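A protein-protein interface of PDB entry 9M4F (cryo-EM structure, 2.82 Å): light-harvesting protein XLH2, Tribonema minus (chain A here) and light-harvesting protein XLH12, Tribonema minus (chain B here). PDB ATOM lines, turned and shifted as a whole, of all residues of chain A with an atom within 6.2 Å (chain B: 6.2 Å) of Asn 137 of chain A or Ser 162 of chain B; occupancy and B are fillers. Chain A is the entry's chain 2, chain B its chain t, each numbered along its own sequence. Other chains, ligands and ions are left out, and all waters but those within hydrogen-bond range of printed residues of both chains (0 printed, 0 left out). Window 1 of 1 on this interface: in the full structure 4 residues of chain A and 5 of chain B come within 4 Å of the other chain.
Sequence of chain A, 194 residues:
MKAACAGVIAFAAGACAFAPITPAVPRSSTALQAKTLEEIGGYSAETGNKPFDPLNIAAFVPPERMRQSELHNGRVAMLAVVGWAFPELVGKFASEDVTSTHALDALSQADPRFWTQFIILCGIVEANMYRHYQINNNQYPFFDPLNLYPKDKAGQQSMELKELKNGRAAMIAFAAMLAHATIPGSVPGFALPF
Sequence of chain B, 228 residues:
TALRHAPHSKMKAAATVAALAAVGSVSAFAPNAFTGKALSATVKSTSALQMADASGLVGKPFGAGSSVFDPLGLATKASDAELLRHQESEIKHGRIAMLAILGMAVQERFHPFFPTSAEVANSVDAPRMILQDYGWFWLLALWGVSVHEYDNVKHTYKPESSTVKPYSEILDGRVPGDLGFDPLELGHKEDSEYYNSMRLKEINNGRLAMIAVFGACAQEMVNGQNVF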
ATOM      1  N   ARG A 131       0.521   9.433  17.917  1.00  0.00           N
ATOM      2  CA  ARG A 131       1.938   9.764  17.967  1.00  0.00           C
ATOM      3  C   ARG A 131       2.738   8.533  18.351  1.00  0.00           C
ATOM      4  O   ARG A 131       3.822   8.285  17.813  1.00  0.00           O
ATOM      5  CB  ARG A 131       2.183  10.894  18.967  1.00  0.00           C
ATOM      6  CG  ARG A 131       3.313  11.831  18.583  1.00  0.00           C
ATOM      7  CD  ARG A 131       3.782  12.653  19.773  1.00  0.00           C
ATOM      8  NE  ARG A 131       2.675  13.291  20.476  1.00  0.00           N
ATOM      9  CZ  ARG A 131       2.076  14.406  20.079  1.00  0.00           C
ATOM     10  NH1 ARG A 131       2.434  15.025  18.968  1.00  0.00           N
ATOM     11  NH2 ARG A 131       1.090  14.909  20.816  1.00  0.00           N
ATOM     12  N   HIS A 132       2.212   7.751  19.287  1.00  0.00           N
ATOM     13  CA  HIS A 132       2.758   6.423  19.536  1.00  0.00           C
ATOM     14  C   HIS A 132       2.208   5.416  18.527  1.00  0.00           C
ATOM     15  O   HIS A 132       1.122   5.589  17.969  1.00  0.00           O
ATOM     16  CB  HIS A 132       2.440   5.951  20.954  1.00  0.00           C
ATOM     17  CG  HIS A 132       3.145   6.727  22.021  1.00  0.00           C
ATOM     18  ND1 HIS A 132       3.532   6.162  23.217  1.00  0.00           N
ATOM     19  CD2 HIS A 132       3.531   8.023  22.074  1.00  0.00           C
ATOM     20  CE1 HIS A 132       4.125   7.078  23.962  1.00  0.00           C
ATOM     21  NE2 HIS A 132       4.138   8.215  23.291  1.00  0.00           N
ATOM     22  N   TYR A 133       2.998   4.375  18.275  1.00  0.00           N
ATOM     23  CA  TYR A 133       2.596   3.208  17.491  1.00  0.00           C
ATOM     24  C   TYR A 133       2.496   3.466  15.992  1.00  0.00           C
ATOM     25  O   TYR A 133       2.378   2.511  15.216  1.00  0.00           O
ATOM     26  CB  TYR A 133       1.239   2.675  17.968  1.00  0.00           C
ATOM     27  CG  TYR A 133       1.199   2.194  19.397  1.00  0.00           C
ATOM     28  CD1 TYR A 133       1.770   0.983  19.757  1.00  0.00           C
ATOM     29  CD2 TYR A 133       0.560   2.934  20.381  1.00  0.00           C
ATOM     30  CE1 TYR A 133       1.725   0.532  21.060  1.00  0.00           C
ATOM     31  CE2 TYR A 133       0.508   2.492  21.687  1.00  0.00           C
ATOM     32  CZ  TYR A 133       1.092   1.290  22.020  1.00  0.00           C
ATOM     33  OH  TYR A 133       1.043   0.845  23.319  1.00  0.00           O
ATOM     34  N   GLN A 134       2.533   4.727  15.557  1.00  0.00           N
ATOM     35  CA  GLN A 134       2.459   5.006  14.126  1.00  0.00           C
ATOM     36  C   GLN A 134       3.348   6.140  13.639  1.00  0.00           C
ATOM     37  O   GLN A 134       3.547   6.241  12.425  1.00  0.00           O
ATOM     38  CB  GLN A 134       1.005   5.291  13.719  1.00  0.00           C
ATOM     39  CG  GLN A 134       0.165   4.023  13.588  1.00  0.00           C
ATOM     40  CD  GLN A 134      -1.325   4.290  13.593  1.00  0.00           C
ATOM     41  OE1 GLN A 134      -1.827   5.040  14.426  1.00  0.00           O
ATOM     42  NE2 GLN A 134      -2.042   3.666  12.667  1.00  0.00           N
ATOM     43  N   ILE A 135       3.887   6.991  14.512  1.00  0.00           N
ATOM     44  CA  ILE A 135       4.796   8.049  14.080  1.00  0.00           C
ATOM     45  C   ILE A 135       6.170   7.793  14.675  1.00  0.00           C
ATOM     46  O   ILE A 135       7.133   7.521  13.951  1.00  0.00           O
ATOM     47  CB  ILE A 135       4.286   9.443  14.495  1.00  0.00           C
ATOM     48  CG1 ILE A 135       2.923   9.741  13.862  1.00  0.00           C
ATOM     49  CG2 ILE A 135       5.305  10.519  14.119  1.00  0.00           C
ATOM     50  CD1 ILE A 135       2.959   9.963  12.360  1.00  0.00           C
ATOM     51  N   ASN A 136       6.266   7.862  16.000  1.00  0.00           N
ATOM     52  CA  ASN A 136       7.534   7.625  16.674  1.00  0.00           C
ATOM     53  C   ASN A 136       7.815   6.147  16.882  1.00  0.00           C
ATOM     54  O   ASN A 136       8.964   5.789  17.161  1.00  0.00           O
ATOM     55  CB  ASN A 136       7.555   8.347  18.022  1.00  0.00           C
ATOM     56  CG  ASN A 136       7.295   9.831  17.886  1.00  0.00           C
ATOM     57  OD1 ASN A 136       7.315  10.373  16.782  1.00  0.00           O
ATOM     58  ND2 ASN A 136       7.053  10.499  19.006  1.00  0.00           N
ATOM     59  N   ASN A 137       6.809   5.289  16.735  1.00  0.00           N
ATOM     60  CA  ASN A 137       6.963   3.855  16.941  1.00  0.00           C
ATOM     61  C   ASN A 137       7.756   3.591  18.219  1.00  0.00           C
ATOM     62  O   ASN A 137       8.837   3.002  18.212  1.00  0.00           O
ATOM     63  CB  ASN A 137       7.623   3.206  15.725  1.00  0.00           C
ATOM     64  CG  ASN A 137       6.868   3.479  14.440  1.00  0.00           C
ATOM     65  OD1 ASN A 137       5.652   3.672  14.451  1.00  0.00           O
ATOM     66  ND2 ASN A 137       7.586   3.502  13.325  1.00  0.00           N
ATOM     67  N   ASN A 138       7.198   4.075  19.330  1.00  0.00           N
ATOM     68  CA  ASN A 138       7.908   4.018  20.602  1.00  0.00           C
ATOM     69  C   ASN A 138       8.071   2.588  21.100  1.00  0.00           C
ATOM     70  O   ASN A 138       9.037   2.292  21.812  1.00  0.00           O
ATOM     71  CB  ASN A 138       7.178   4.876  21.633  1.00  0.00           C
ATOM     72  CG  ASN A 138       7.536   6.348  21.523  1.00  0.00           C
ATOM     73  OD1 ASN A 138       8.298   6.748  20.645  1.00  0.00           O
ATOM     74  ND2 ASN A 138       6.981   7.160  22.412  1.00  0.00           N
ATOM     75  N   GLN A 139       7.148   1.697  20.751  1.00  0.00           N
ATOM     76  CA  GLN A 139       7.228   0.270  21.047  1.00  0.00           C
ATOM     77  C   GLN A 139       7.116  -0.042  22.533  1.00  0.00           C
ATOM     78  O   GLN A 139       7.355  -1.188  22.935  1.00  0.00           O
ATOM     79  CB  GLN A 139       8.522  -0.345  20.500  1.00  0.00           C
ATOM     80  CG  GLN A 139       8.693  -0.171  19.002  1.00  0.00           C
ATOM     81  CD  GLN A 139       7.600  -0.857  18.206  1.00  0.00           C
ATOM     82  OE1 GLN A 139       7.081  -1.897  18.611  1.00  0.00           O
ATOM     83  NE2 GLN A 139       7.241  -0.273  17.069  1.00  0.00           N
ATOM     84  N   TYR A 140       6.768   0.939  23.364  1.00  0.00           N
ATOM     85  CA  TYR A 140       6.429   0.683  24.752  1.00  0.00           C
ATOM     86  C   TYR A 140       5.035   1.229  25.035  1.00  0.00           C
ATOM     87  O   TYR A 140       4.608   2.199  24.399  1.00  0.00           O
ATOM     88  CB  TYR A 140       7.441   1.315  25.718  1.00  0.00           C
ATOM     89  CG  TYR A 140       7.762   2.765  25.440  1.00  0.00           C
ATOM     90  CD1 TYR A 140       6.910   3.778  25.854  1.00  0.00           C
ATOM     91  CD2 TYR A 140       8.927   3.121  24.778  1.00  0.00           C
ATOM     92  CE1 TYR A 140       7.204   5.103  25.607  1.00  0.00           C
ATOM     93  CE2 TYR A 140       9.230   4.444  24.527  1.00  0.00           C
ATOM     94  CZ  TYR A 140       8.365   5.431  24.945  1.00  0.00           C
ATOM     95  OH  TYR A 140       8.660   6.750  24.696  1.00  0.00           O
ATOM     96  N   GLU B 160      12.846  10.745  24.705  1.00  0.00           N
ATOM     97  CA  GLU B 160      12.395   9.531  24.036  1.00  0.00           C
ATOM     98  C   GLU B 160      13.146   9.338  22.724  1.00  0.00           C
ATOM     99  O   GLU B 160      13.331  10.282  21.950  1.00  0.00           O
ATOM    100  CB  GLU B 160      10.893   9.589  23.758  1.00  0.00           C
ATOM    101  CG  GLU B 160      10.021   9.879  24.970  1.00  0.00           C
ATOM    102  CD  GLU B 160       9.840  11.363  25.213  1.00  0.00           C
ATOM    103  OE1 GLU B 160      10.836  12.109  25.107  1.00  0.00           O
ATOM    104  OE2 GLU B 160       8.700  11.786  25.497  1.00  0.00           O
ATOM    105  N   SER B 161      13.585   8.107  22.478  1.00  0.00           N
ATOM    106  CA  SER B 161      14.310   7.758  21.258  1.00  0.00           C
ATOM    107  C   SER B 161      13.852   6.393  20.750  1.00  0.00           C
ATOM    108  O   SER B 161      14.660   5.534  20.394  1.00  0.00           O
ATOM    109  CB  SER B 161      15.817   7.776  21.503  1.00  0.00           C
ATOM    110  OG  SER B 161      16.531   7.462  20.321  1.00  0.00           O
ATOM    111  N   SER B 162      12.537   6.177  20.721  1.00  0.00           N
ATOM    112  CA  SER B 162      11.900   4.883  20.483  1.00  0.00           C
ATOM    113  C   SER B 162      12.054   3.964  21.684  1.00  0.00           C
ATOM    114  O   SER B 162      11.587   2.820  21.645  1.00  0.00           O
ATOM    115  CB  SER B 162      12.447   4.170  19.237  1.00  0.00           C
ATOM    116  OG  SER B 162      12.379   5.009  18.097  1.00  0.00           O
ATOM    117  N   THR B 163      12.684   4.430  22.768  1.00  0.00           N
ATOM    118  CA  THR B 163      12.919   3.660  24.019  1.00  0.00           C
ATOM    119  C   THR B 163      12.927   4.723  25.125  1.00  0.00           C
ATOM    120  O   THR B 163      12.245   5.741  24.911  1.00  0.00           O
ATOM    121  CB  THR B 163      14.216   2.844  23.928  1.00  0.00           C
ATOM    122  OG1 THR B 163      15.294   3.765  23.765  1.00  0.00           O
ATOM    123  CG2 THR B 163      14.246   1.844  22.791  1.00  0.00           C
ATOM    124  N   VAL B 164      13.637   4.540  26.244  1.00  0.00           N
ATOM    125  CA  VAL B 164      13.785   5.589  27.301  1.00  0.00           C
ATOM    126  C   VAL B 164      12.386   6.169  27.533  1.00  0.00           C
ATOM    127  O   VAL B 164      12.154   7.324  27.128  1.00  0.00           O
ATOM    128  CB  VAL B 164      14.890   6.634  27.004  1.00  0.00           C
ATOM    129  CG1 VAL B 164      16.264   5.982  26.969  1.00  0.00           C
ATOM    130  CG2 VAL B 164      14.664   7.436  25.731  1.00  0.00           C
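O of Ser 162 of chain B sits close to O of Asn 138 of chain A.
Among the printed residues, pairs that only touch across the chains: Tyr 140 of chain A with Thr 163 of chain B (3.3 Å), Tyr 140 of chain A with Glu 160 of chain B (3.4 Å), Asn 136 of chain A with Ser 162 of chain B (3.6 Å) and Asn 137 of chain A with Ser 162 of chain B (3.9 Å).
Asn 137 of chain A touches just one residue of chain B: Ser 162. Printed residues of chain B within 4 Å of Asn 138 of chain A: Ser 162 (2.6 Å). Of the printed residues of chain B, Tyr 140 of chain A touches Glu 160 and Thr 163. Of the printed residues of chain A, Ser 162 of chain B touches Asn 136 (3.6 Å), Asn 137 (3.9 Å) and Asn 138 (2.6 Å). The nearest residue of chain B that does not touch Asn 137 of chain A is Thr 163 of chain B (6.1 Å). The nearest residue of chain A that does not touch Ser 162 of chain B is Tyr 140 of chain A (4.04 Å).
O of Arg 131 of chain A lies within hydrogen-bond range of N of Asn 136 of chain A (3.1 Å). The side-chain amide nitrogen of Asn 138 of chain A is in hydrogen-bond range of a ring nitrogen (NE2) of His 132 of chain A, 3.2 Å away. The backbone NH of Gln 134 of chain A lies close to the side-chain amide oxygen of Asn 137 of chain A (3.5 Å). OH of Tyr 140 of chain A sits at hydrogen-bond distance from ND2 of Asn 138 of chain A.
Of the 10 printed residues of chain A, 4 touch a printed residue of chain B. Along chain A the printed residues that touch a printed residue of chain B span positions 136 to 140. Among the printed residues, 5 pairs touch across the chains. Among the printed residues, no Asp or Glu carboxylate lies within 4 Å of a Lys or Arg side-chain nitrogen of the other chain.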
